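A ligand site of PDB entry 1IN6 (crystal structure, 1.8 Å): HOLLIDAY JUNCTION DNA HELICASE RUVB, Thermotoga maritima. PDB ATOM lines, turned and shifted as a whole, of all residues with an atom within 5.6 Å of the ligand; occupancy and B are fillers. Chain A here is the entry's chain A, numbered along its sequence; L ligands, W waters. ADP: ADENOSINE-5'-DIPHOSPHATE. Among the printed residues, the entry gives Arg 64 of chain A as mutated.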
ATOM      1  N   LEU A  19      16.277  25.652   2.933  1.00  0.00           N
ATOM      2  CA  LEU A  19      14.927  25.091   2.870  1.00  0.00           C
ATOM      3  C   LEU A  19      14.040  25.823   1.875  1.00  0.00           C
ATOM      4  O   LEU A  19      12.874  25.463   1.704  1.00  0.00           O
ATOM      5  CB  LEU A  19      14.277  25.119   4.258  1.00  0.00           C
ATOM      6  CG  LEU A  19      14.946  24.254   5.328  1.00  0.00           C
ATOM      7  CD1 LEU A  19      14.459  24.681   6.697  1.00  0.00           C
ATOM      8  CD2 LEU A  19      14.647  22.790   5.075  1.00  0.00           C
ATOM      9  N   ARG A  20      14.581  26.839   1.233  1.00  0.00           N
ATOM     10  CA  ARG A  20      13.820  27.631   0.266  1.00  0.00           C
ATOM     11  C   ARG A  20      13.947  27.099  -1.164  1.00  0.00           C
ATOM     12  O   ARG A  20      15.048  26.932  -1.669  1.00  0.00           O
ATOM     13  CB  ARG A  20      14.275  29.101   0.317  1.00  0.00           C
ATOM     14  CG  ARG A  20      13.388  30.069  -0.462  1.00  0.00           C
ATOM     15  CD  ARG A  20      13.963  31.481  -0.487  1.00  0.00           C
ATOM     16  NE  ARG A  20      13.961  32.122   0.830  1.00  0.00           N
ATOM     17  CZ  ARG A  20      12.871  32.605   1.421  1.00  0.00           C
ATOM     18  NH1 ARG A  20      11.690  32.526   0.825  1.00  0.00           N
ATOM     19  NH2 ARG A  20      12.960  33.170   2.617  1.00  0.00           N
ATOM     20  N   PRO A  21      12.805  26.820  -1.820  1.00  0.00           N
ATOM     21  CA  PRO A  21      12.792  26.315  -3.199  1.00  0.00           C
ATOM     22  C   PRO A  21      13.623  27.212  -4.103  1.00  0.00           C
ATOM     23  O   PRO A  21      13.501  28.438  -4.045  1.00  0.00           O
ATOM     24  CB  PRO A  21      11.314  26.354  -3.558  1.00  0.00           C
ATOM     25  CG  PRO A  21      10.658  26.021  -2.278  1.00  0.00           C
ATOM     26  CD  PRO A  21      11.436  26.863  -1.270  1.00  0.00           C
ATOM     27  N   GLU A  26      10.895  22.703  -7.536  1.00  0.00           N
ATOM     28  CA  GLU A  26      11.057  22.463  -6.105  1.00  0.00           C
ATOM     29  C   GLU A  26       9.945  23.102  -5.288  1.00  0.00           C
ATOM     30  O   GLU A  26       9.861  22.898  -4.073  1.00  0.00           O
ATOM     31  CB  GLU A  26      12.412  22.994  -5.621  1.00  0.00           C
ATOM     32  CG  GLU A  26      13.607  22.350  -6.284  1.00  0.00           C
ATOM     33  CD  GLU A  26      14.928  22.865  -5.755  1.00  0.00           C
ATOM     34  OE1 GLU A  26      15.980  22.455  -6.289  1.00  0.00           O
ATOM     35  OE2 GLU A  26      14.929  23.688  -4.819  1.00  0.00           O
ATOM     36  N   PHE A  27       9.117  23.892  -5.949  1.00  0.00           N
ATOM     37  CA  PHE A  27       8.015  24.591  -5.298  1.00  0.00           C
ATOM     38  C   PHE A  27       6.787  23.691  -5.258  1.00  0.00           C
ATOM     39  O   PHE A  27       6.163  23.444  -6.282  1.00  0.00           O
ATOM     40  CB  PHE A  27       7.729  25.892  -6.054  1.00  0.00           C
ATOM     41  CG  PHE A  27       6.925  26.905  -5.282  1.00  0.00           C
ATOM     42  CD1 PHE A  27       5.532  26.839  -5.273  1.00  0.00           C
ATOM     43  CD2 PHE A  27       7.560  27.940  -4.610  1.00  0.00           C
ATOM     44  CE1 PHE A  27       4.784  27.810  -4.592  1.00  0.00           C
ATOM     45  CE2 PHE A  27       6.823  28.906  -3.923  1.00  0.00           C
ATOM     46  CZ  PHE A  27       5.429  28.848  -3.919  1.00  0.00           C
ATOM     47  N   ILE A  28       6.474  23.174  -4.076  1.00  0.00           N
ATOM     48  CA  ILE A  28       5.327  22.282  -3.901  1.00  0.00           C
ATOM     49  C   ILE A  28       3.979  23.012  -3.868  1.00  0.00           C
ATOM     50  O   ILE A  28       3.889  24.107  -3.329  1.00  0.00           O
ATOM     51  CB  ILE A  28       5.472  21.459  -2.618  1.00  0.00           C
ATOM     52  CG1 ILE A  28       6.709  20.560  -2.735  1.00  0.00           C
ATOM     53  CG2 ILE A  28       4.217  20.655  -2.356  1.00  0.00           C
ATOM     54  CD1 ILE A  28       7.108  19.887  -1.445  1.00  0.00           C
ATOM     55  N   GLY A  29       2.950  22.396  -4.437  1.00  0.00           N
ATOM     56  CA  GLY A  29       1.635  23.013  -4.430  1.00  0.00           C
ATOM     57  C   GLY A  29       1.523  24.220  -5.344  1.00  0.00           C
ATOM     58  O   GLY A  29       2.395  24.457  -6.178  1.00  0.00           O
ATOM     59  N   GLN A  30       0.440  24.975  -5.179  1.00  0.00           N
ATOM     60  CA  GLN A  30       0.192  26.168  -5.996  1.00  0.00           C
ATOM     61  C   GLN A  30       0.267  25.841  -7.499  1.00  0.00           C
ATOM     62  O   GLN A  30       0.869  26.580  -8.283  1.00  0.00           O
ATOM     63  CB  GLN A  30       1.208  27.276  -5.682  1.00  0.00           C
ATOM     64  CG  GLN A  30       1.147  27.834  -4.247  1.00  0.00           C
ATOM     65  CD  GLN A  30      -0.236  28.305  -3.838  1.00  0.00           C
ATOM     66  OE1 GLN A  30      -1.011  28.786  -4.674  1.00  0.00           O
ATOM     67  NE2 GLN A  30      -0.551  28.185  -2.547  1.00  0.00           N
ATOM     68  N   PRO A  59      -1.735  35.802   1.930  1.00  0.00           N
ATOM     69  CA  PRO A  59      -1.251  35.975   3.299  1.00  0.00           C
ATOM     70  C   PRO A  59       0.226  35.593   3.415  1.00  0.00           C
ATOM     71  O   PRO A  59       0.760  34.865   2.572  1.00  0.00           O
ATOM     72  CB  PRO A  59      -2.168  35.063   4.117  1.00  0.00           C
ATOM     73  CG  PRO A  59      -2.576  34.014   3.146  1.00  0.00           C
ATOM     74  CD  PRO A  59      -2.817  34.800   1.867  1.00  0.00           C
ATOM     75  N   PRO A  60       0.900  36.088   4.454  1.00  0.00           N
ATOM     76  CA  PRO A  60       2.329  35.815   4.698  1.00  0.00           C
ATOM     77  C   PRO A  60       2.687  34.339   4.869  1.00  0.00           C
ATOM     78  O   PRO A  60       1.877  33.534   5.350  1.00  0.00           O
ATOM     79  CB  PRO A  60       2.620  36.613   5.960  1.00  0.00           C
ATOM     80  CG  PRO A  60       1.626  37.713   5.928  1.00  0.00           C
ATOM     81  CD  PRO A  60       0.374  37.005   5.470  1.00  0.00           C
ATOM     82  N   GLY A  61       3.910  33.990   4.480  1.00  0.00           N
ATOM     83  CA  GLY A  61       4.402  32.628   4.607  1.00  0.00           C
ATOM     84  C   GLY A  61       3.939  31.641   3.555  1.00  0.00           C
ATOM     85  O   GLY A  61       4.157  30.443   3.706  1.00  0.00           O
ATOM     86  N   LEU A  62       3.329  32.147   2.487  1.00  0.00           N
ATOM     87  CA  LEU A  62       2.814  31.294   1.421  1.00  0.00           C
ATOM     88  C   LEU A  62       3.754  31.111   0.230  1.00  0.00           C
ATOM     89  O   LEU A  62       3.447  30.380  -0.700  1.00  0.00           O
ATOM     90  CB  LEU A  62       1.480  31.837   0.927  1.00  0.00           C
ATOM     91  CG  LEU A  62       0.293  31.777   1.883  1.00  0.00           C
ATOM     92  CD1 LEU A  62      -0.965  32.103   1.058  1.00  0.00           C
ATOM     93  CD2 LEU A  62       0.149  30.401   2.508  1.00  0.00           C
ATOM     94  N   GLY A  63       4.875  31.826   0.242  1.00  0.00           N
ATOM     95  CA  GLY A  63       5.829  31.684  -0.839  1.00  0.00           C
ATOM     96  C   GLY A  63       6.001  32.830  -1.803  1.00  0.00           C
ATOM     97  O   GLY A  63       6.600  32.638  -2.866  1.00  0.00           O
ATOM     98  N   ARG A  64       5.467  34.004  -1.487  1.00  0.00           N
ATOM     99  CA  ARG A  64       5.609  35.145  -2.388  1.00  0.00           C
ATOM    100  C   ARG A  64       7.084  35.517  -2.621  1.00  0.00           C
ATOM    101  O   ARG A  64       7.517  35.659  -3.763  1.00  0.00           O
ATOM    102  CB  ARG A  64       4.816  36.335  -1.842  1.00  0.00           C
ATOM    103  CG  ARG A  64       3.295  36.050  -1.793  1.00  0.00           C
ATOM    104  CD  ARG A  64       2.587  36.998  -0.856  1.00  0.00           C
ATOM    105  NE  ARG A  64       3.201  36.979   0.463  1.00  0.00           N
ATOM    106  CZ  ARG A  64       3.158  37.976   1.332  1.00  0.00           C
ATOM    107  NH1 ARG A  64       2.516  39.095   1.019  1.00  0.00           N
ATOM    108  NH2 ARG A  64       3.777  37.864   2.502  1.00  0.00           N
ATOM    109  N   THR A  65       7.840  35.665  -1.544  1.00  0.00           N
ATOM    110  CA  THR A  65       9.261  36.001  -1.636  1.00  0.00           C
ATOM    111  C   THR A  65      10.002  34.895  -2.390  1.00  0.00           C
ATOM    112  O   THR A  65      10.885  35.158  -3.200  1.00  0.00           O
ATOM    113  CB  THR A  65       9.884  36.169  -0.213  1.00  0.00           C
ATOM    114  OG1 THR A  65       9.364  37.351   0.403  1.00  0.00           O
ATOM    115  CG2 THR A  65      11.405  36.310  -0.293  1.00  0.00           C
ATOM    116  N   THR A  66       9.634  33.656  -2.095  1.00  0.00           N
ATOM    117  CA  THR A  66      10.247  32.496  -2.742  1.00  0.00           C
ATOM    118  C   THR A  66      10.053  32.582  -4.253  1.00  0.00           C
ATOM    119  O   THR A  66      11.000  32.402  -5.027  1.00  0.00           O
ATOM    120  CB  THR A  66       9.634  31.199  -2.186  1.00  0.00           C
ATOM    121  OG1 THR A  66       9.934  31.093  -0.785  1.00  0.00           O
ATOM    122  CG2 THR A  66      10.177  29.995  -2.911  1.00  0.00           C
ATOM    123  N   LEU A  67       8.828  32.864  -4.687  1.00  0.00           N
ATOM    124  CA  LEU A  67       8.543  32.968  -6.118  1.00  0.00           C
ATOM    125  C   LEU A  67       9.278  34.129  -6.767  1.00  0.00           C
ATOM    126  O   LEU A  67       9.703  34.019  -7.922  1.00  0.00           O
ATOM    127  CB  LEU A  67       7.041  33.108  -6.350  1.00  0.00           C
ATOM    128  CG  LEU A  67       6.255  31.820  -6.101  1.00  0.00           C
ATOM    129  CD1 LEU A  67       4.774  32.135  -6.150  1.00  0.00           C
ATOM    130  CD2 LEU A  67       6.614  30.754  -7.146  1.00  0.00           C
ATOM    131  N   PHE A 107      11.887  43.588  -6.829  1.00  0.00           N
ATOM    132  CA  PHE A 107      10.933  42.967  -5.915  1.00  0.00           C
ATOM    133  C   PHE A 107      10.601  43.901  -4.761  1.00  0.00           C
ATOM    134  O   PHE A 107      11.496  44.317  -4.013  1.00  0.00           O
ATOM    135  CB  PHE A 107      11.474  41.650  -5.368  1.00  0.00           C
ATOM    136  CG  PHE A 107      10.610  41.034  -4.304  1.00  0.00           C
ATOM    137  CD1 PHE A 107       9.272  40.748  -4.561  1.00  0.00           C
ATOM    138  CD2 PHE A 107      11.139  40.733  -3.051  1.00  0.00           C
ATOM    139  CE1 PHE A 107       8.465  40.165  -3.579  1.00  0.00           C
ATOM    140  CE2 PHE A 107      10.350  40.155  -2.066  1.00  0.00           C
ATOM    141  CZ  PHE A 107       9.003  39.866  -2.325  1.00  0.00           C
ATOM    142  N   ASP A 109       8.250  44.057  -1.491  1.00  0.00           N
ATOM    143  CA  ASP A 109       7.352  43.409  -0.558  1.00  0.00           C
ATOM    144  C   ASP A 109       6.455  44.483   0.040  1.00  0.00           C
ATOM    145  O   ASP A 109       6.857  45.642   0.131  1.00  0.00           O
ATOM    146  CB  ASP A 109       8.158  42.698   0.519  1.00  0.00           C
ATOM    147  CG  ASP A 109       7.283  41.994   1.532  1.00  0.00           C
ATOM    148  OD1 ASP A 109       6.316  41.331   1.110  1.00  0.00           O
ATOM    149  OD2 ASP A 109       7.588  42.106   2.743  1.00  0.00           O
ATOM    150  N   TYR A 180      -2.412  26.375   1.448  1.00  0.00           N
ATOM    151  CA  TYR A 180      -2.081  25.080   0.894  1.00  0.00           C
ATOM    152  C   TYR A 180      -2.938  23.990   1.541  1.00  0.00           C
ATOM    153  O   TYR A 180      -3.438  24.176   2.648  1.00  0.00           O
ATOM    154  CB  TYR A 180      -0.613  24.734   1.140  1.00  0.00           C
ATOM    155  CG  TYR A 180       0.376  25.583   0.374  1.00  0.00           C
ATOM    156  CD1 TYR A 180       0.522  26.945   0.636  1.00  0.00           C
ATOM    157  CD2 TYR A 180       1.203  25.009  -0.592  1.00  0.00           C
ATOM    158  CE1 TYR A 180       1.476  27.715  -0.053  1.00  0.00           C
ATOM    159  CE2 TYR A 180       2.150  25.760  -1.273  1.00  0.00           C
ATOM    160  CZ  TYR A 180       2.290  27.102  -1.003  1.00  0.00           C
ATOM    161  OH  TYR A 180       3.250  27.838  -1.672  1.00  0.00           O
ATOM    162  N   ILE A 188       5.729  19.255   2.028  1.00  0.00           N
ATOM    163  CA  ILE A 188       6.708  20.295   2.355  1.00  0.00           C
ATOM    164  C   ILE A 188       7.386  19.941   3.677  1.00  0.00           C
ATOM    165  O   ILE A 188       8.595  20.165   3.860  1.00  0.00           O
ATOM    166  CB  ILE A 188       6.010  21.676   2.448  1.00  0.00           C
ATOM    167  CG1 ILE A 188       5.602  22.125   1.050  1.00  0.00           C
ATOM    168  CG2 ILE A 188       6.937  22.719   3.107  1.00  0.00           C
ATOM    169  CD1 ILE A 188       4.774  23.399   1.011  1.00  0.00           C
ATOM    170  N   ARG A 191       9.853  17.121   3.210  1.00  0.00           N
ATOM    171  CA  ARG A 191      11.020  17.639   2.502  1.00  0.00           C
ATOM    172  C   ARG A 191      11.934  18.378   3.473  1.00  0.00           C
ATOM    173  O   ARG A 191      13.158  18.213   3.453  1.00  0.00           O
ATOM    174  CB  ARG A 191      10.564  18.571   1.365  1.00  0.00           C
ATOM    175  CG  ARG A 191      11.685  19.350   0.661  1.00  0.00           C
ATOM    176  CD  ARG A 191      11.118  20.248  -0.444  1.00  0.00           C
ATOM    177  NE  ARG A 191      12.147  20.989  -1.166  1.00  0.00           N
ATOM    178  CZ  ARG A 191      12.701  22.127  -0.744  1.00  0.00           C
ATOM    179  NH1 ARG A 191      13.644  22.722  -1.474  1.00  0.00           N
ATOM    180  NH2 ARG A 191      12.291  22.686   0.383  1.00  0.00           N
ATOM    181  N   PRO A 216       3.130  27.289   4.582  1.00  0.00           N
ATOM    182  CA  PRO A 216       4.463  26.661   4.551  1.00  0.00           C
ATOM    183  C   PRO A 216       5.371  27.162   5.677  1.00  0.00           C
ATOM    184  O   PRO A 216       5.996  26.371   6.373  1.00  0.00           O
ATOM    185  CB  PRO A 216       4.973  27.060   3.162  1.00  0.00           C
ATOM    186  CG  PRO A 216       3.722  26.990   2.332  1.00  0.00           C
ATOM    187  CD  PRO A 216       2.695  27.691   3.235  1.00  0.00           C
ATOM    188  N   ARG A 217       5.449  28.472   5.865  1.00  0.00           N
ATOM    189  CA  ARG A 217       6.300  29.039   6.918  1.00  0.00           C
ATOM    190  C   ARG A 217       6.036  28.386   8.275  1.00  0.00           C
ATOM    191  O   ARG A 217       6.970  27.975   8.981  1.00  0.00           O
ATOM    192  CB  ARG A 217       6.072  30.536   7.016  1.00  0.00           C
ATOM    193  CG  ARG A 217       6.692  31.165   8.249  1.00  0.00           C
ATOM    194  CD  ARG A 217       6.528  32.682   8.240  1.00  0.00           C
ATOM    195  NE  ARG A 217       7.431  33.289   7.273  1.00  0.00           N
ATOM    196  CZ  ARG A 217       7.262  34.491   6.739  1.00  0.00           C
ATOM    197  NH1 ARG A 217       6.219  35.231   7.073  1.00  0.00           N
ATOM    198  NH2 ARG A 217       8.150  34.937   5.861  1.00  0.00           N
ATOM    199  N   ILE A 220       7.022  24.585   8.466  1.00  0.00           N
ATOM    200  CA  ILE A 220       8.479  24.418   8.560  1.00  0.00           C
ATOM    201  C   ILE A 220       9.019  24.734   9.942  1.00  0.00           C
ATOM    202  O   ILE A 220       9.912  24.032  10.449  1.00  0.00           O
ATOM    203  CB  ILE A 220       9.173  25.287   7.504  1.00  0.00           C
ATOM    204  CG1 ILE A 220       8.834  24.757   6.114  1.00  0.00           C
ATOM    205  CG2 ILE A 220      10.676  25.308   7.734  1.00  0.00           C
ATOM    206  CD1 ILE A 220       9.242  25.683   4.995  1.00  0.00           C
HETATM  207  PB  ADP L   1       6.016  35.098   1.932  1.00  0.00           P
HETATM  208  O1B ADP L   1       4.783  34.779   1.188  1.00  0.00           O
HETATM  209  O2B ADP L   1       6.939  36.079   1.173  1.00  0.00           O
HETATM  210  O3B ADP L   1       5.709  35.663   3.328  1.00  0.00           O
HETATM  211  PA  ADP L   1       8.214  33.142   1.851  1.00  0.00           P
HETATM  212  O1A ADP L   1       8.425  33.080   0.391  1.00  0.00           O
HETATM  213  O2A ADP L   1       9.260  33.888   2.566  1.00  0.00           O
HETATM  214  O3A ADP L   1       6.749  33.778   2.187  1.00  0.00           O
HETATM  215  O5' ADP L   1       8.099  31.690   2.477  1.00  0.00           O
HETATM  216  C5' ADP L   1       8.130  31.062   3.709  1.00  0.00           C
HETATM  217  C4' ADP L   1       8.941  29.986   3.943  1.00  0.00           C
HETATM  218  O4' ADP L   1       8.201  28.915   3.468  1.00  0.00           O
HETATM  219  C3' ADP L   1      10.169  29.868   3.009  1.00  0.00           C
HETATM  220  O3' ADP L   1      11.049  29.354   3.961  1.00  0.00           O
HETATM  221  C2' ADP L   1      10.050  28.826   2.047  1.00  0.00           C
HETATM  222  O2' ADP L   1      11.383  28.396   1.685  1.00  0.00           O
HETATM  223  C1' ADP L   1       8.635  28.192   2.455  1.00  0.00           C
HETATM  224  N9  ADP L   1       7.809  27.957   1.368  1.00  0.00           N
HETATM  225  C8  ADP L   1       6.887  28.778   0.792  1.00  0.00           C
HETATM  226  N7  ADP L   1       6.285  28.281  -0.168  1.00  0.00           N
HETATM  227  C5  ADP L   1       6.813  27.022  -0.303  1.00  0.00           C
HETATM  228  C6  ADP L   1       6.567  25.911  -1.207  1.00  0.00           C
HETATM  229  N6  ADP L   1       5.624  26.030  -2.184  1.00  0.00           N
HETATM  230  N1  ADP L   1       7.304  24.701  -1.087  1.00  0.00           N
HETATM  231  C2  ADP L   1       8.260  24.591  -0.076  1.00  0.00           C
HETATM  232  N3  ADP L   1       8.552  25.599   0.836  1.00  0.00           N
HETATM  233  C4  ADP L   1       7.795  26.792   0.672  1.00  0.00           C
HETATM  234  O   HOH W   1      13.942  29.096   4.022  1.00  0.00           O
HETATM  235  O   HOH W   2      10.584  24.527   2.330  1.00  0.00           O
HETATM  236  O   HOH W   3       9.715  36.857   3.730  1.00  0.00           O
HETATM  237  O   HOH W   4       6.804  38.815   0.330  1.00  0.00           O
HETATM  238  O   HOH W   5       6.775  37.454   4.894  1.00  0.00           O
HETATM  239  O   HOH W   6      10.866  29.787   7.057  1.00  0.00           O
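Residues that only touch the ligand: Pro 21, Phe 27, Pro 60, Ile 188, Pro 216 and Ile 220. 17 residues have an atom within 4 Å of the ligand: Leu 19, Arg 20, Pro 21, Phe 27, Ile 28, Pro 60, Gly 61, Leu 62, Gly 63, Arg 64, Thr 65, Thr 66, Tyr 180, Ile 188, Pro 216, Arg 217 and Ile 220.
O3B of the ligand is in hydrogen-bond range of N of Gly 61, at 2.7 Å. An oxygen (O1A) of the ligand lies within hydrogen-bond range of the backbone NH (N) of Thr 66. An oxygen (O1A) of the ligand is in hydrogen-bond range of the side-chain hydroxyl of Thr 66 (2.8 Å). N of Arg 64 sits at hydrogen-bond distance from O1B of the ligand, 2.9 Å away. O1B of the ligand is in salt-bridge range of NE of Arg 64 (2.8 Å). The backbone NH (N) of Ile 28 lies within hydrogen-bond range of a nitrogen (N1) of the ligand. The backbone carbonyl oxygen (O) of Ile 28 lies within hydrogen-bond range of a nitrogen (N6) of the ligand, 2.8 Å away. An oxygen (O2B) of the ligand is in hydrogen-bond range of the backbone NH (N) of Thr 65, at 2.9 Å. OG1 of Thr 65 is in hydrogen-bond range of O2B of the ligand, 2.8 Å away. An oxygen (O2A) of the ligand lies within salt-bridge range of the guanidinium group (NH1) of Arg 20. The side-chain hydroxyl of Tyr 180 sits at hydrogen-bond distance from a nitrogen (N6) of the ligand, 3.0 Å away. An oxygen (O1B) of the ligand lies within hydrogen-bond range of the backbone NH of Gly 63. O1B of the ligand is in hydrogen-bond range of N of Leu 62. O of Leu 19 is in hydrogen-bond range of O2' of the ligand. O3B of the ligand is in salt-bridge range of NH2 of Arg 217, at 3.6 Å.
The backbone carbonyl oxygen (O) of Gly 61 sits at hydrogen-bond distance from the backbone NH (N) of Arg 217. The guanidinium group (NH1) of Arg 20 lies within hydrogen-bond range of the side-chain hydroxyl (OG1) of Thr 66 (2.8 Å). The side-chain hydroxyl (OH) of Tyr 180 lies within hydrogen-bond range of the backbone carbonyl oxygen (O) of Leu 62, at 2.7 Å. The backbone carbonyl oxygen (O) of Leu 19 sits at hydrogen-bond distance from the guanidinium group (NH2) of Arg 191.
Water W5 bridges an oxygen (O3B) of the ligand and the guanidinium group (NH2) of Arg 217. Water W2 lies within hydrogen-bond range of the backbone carbonyl oxygen of Leu 19, a nitrogen (N3) of the ligand and the guanidinium group of Arg 191. Water W4 lies within hydrogen-bond range of the side-chain carboxylate (OD1) of Asp 109, an oxygen (O2B) of the ligand and the side-chain hydroxyl (OG1) of Thr 65. Water W3 lies within hydrogen-bond range of an oxygen (O2A) of the ligand, the guanidinium group of Arg 217 and the side-chain hydroxyl of Thr 65.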
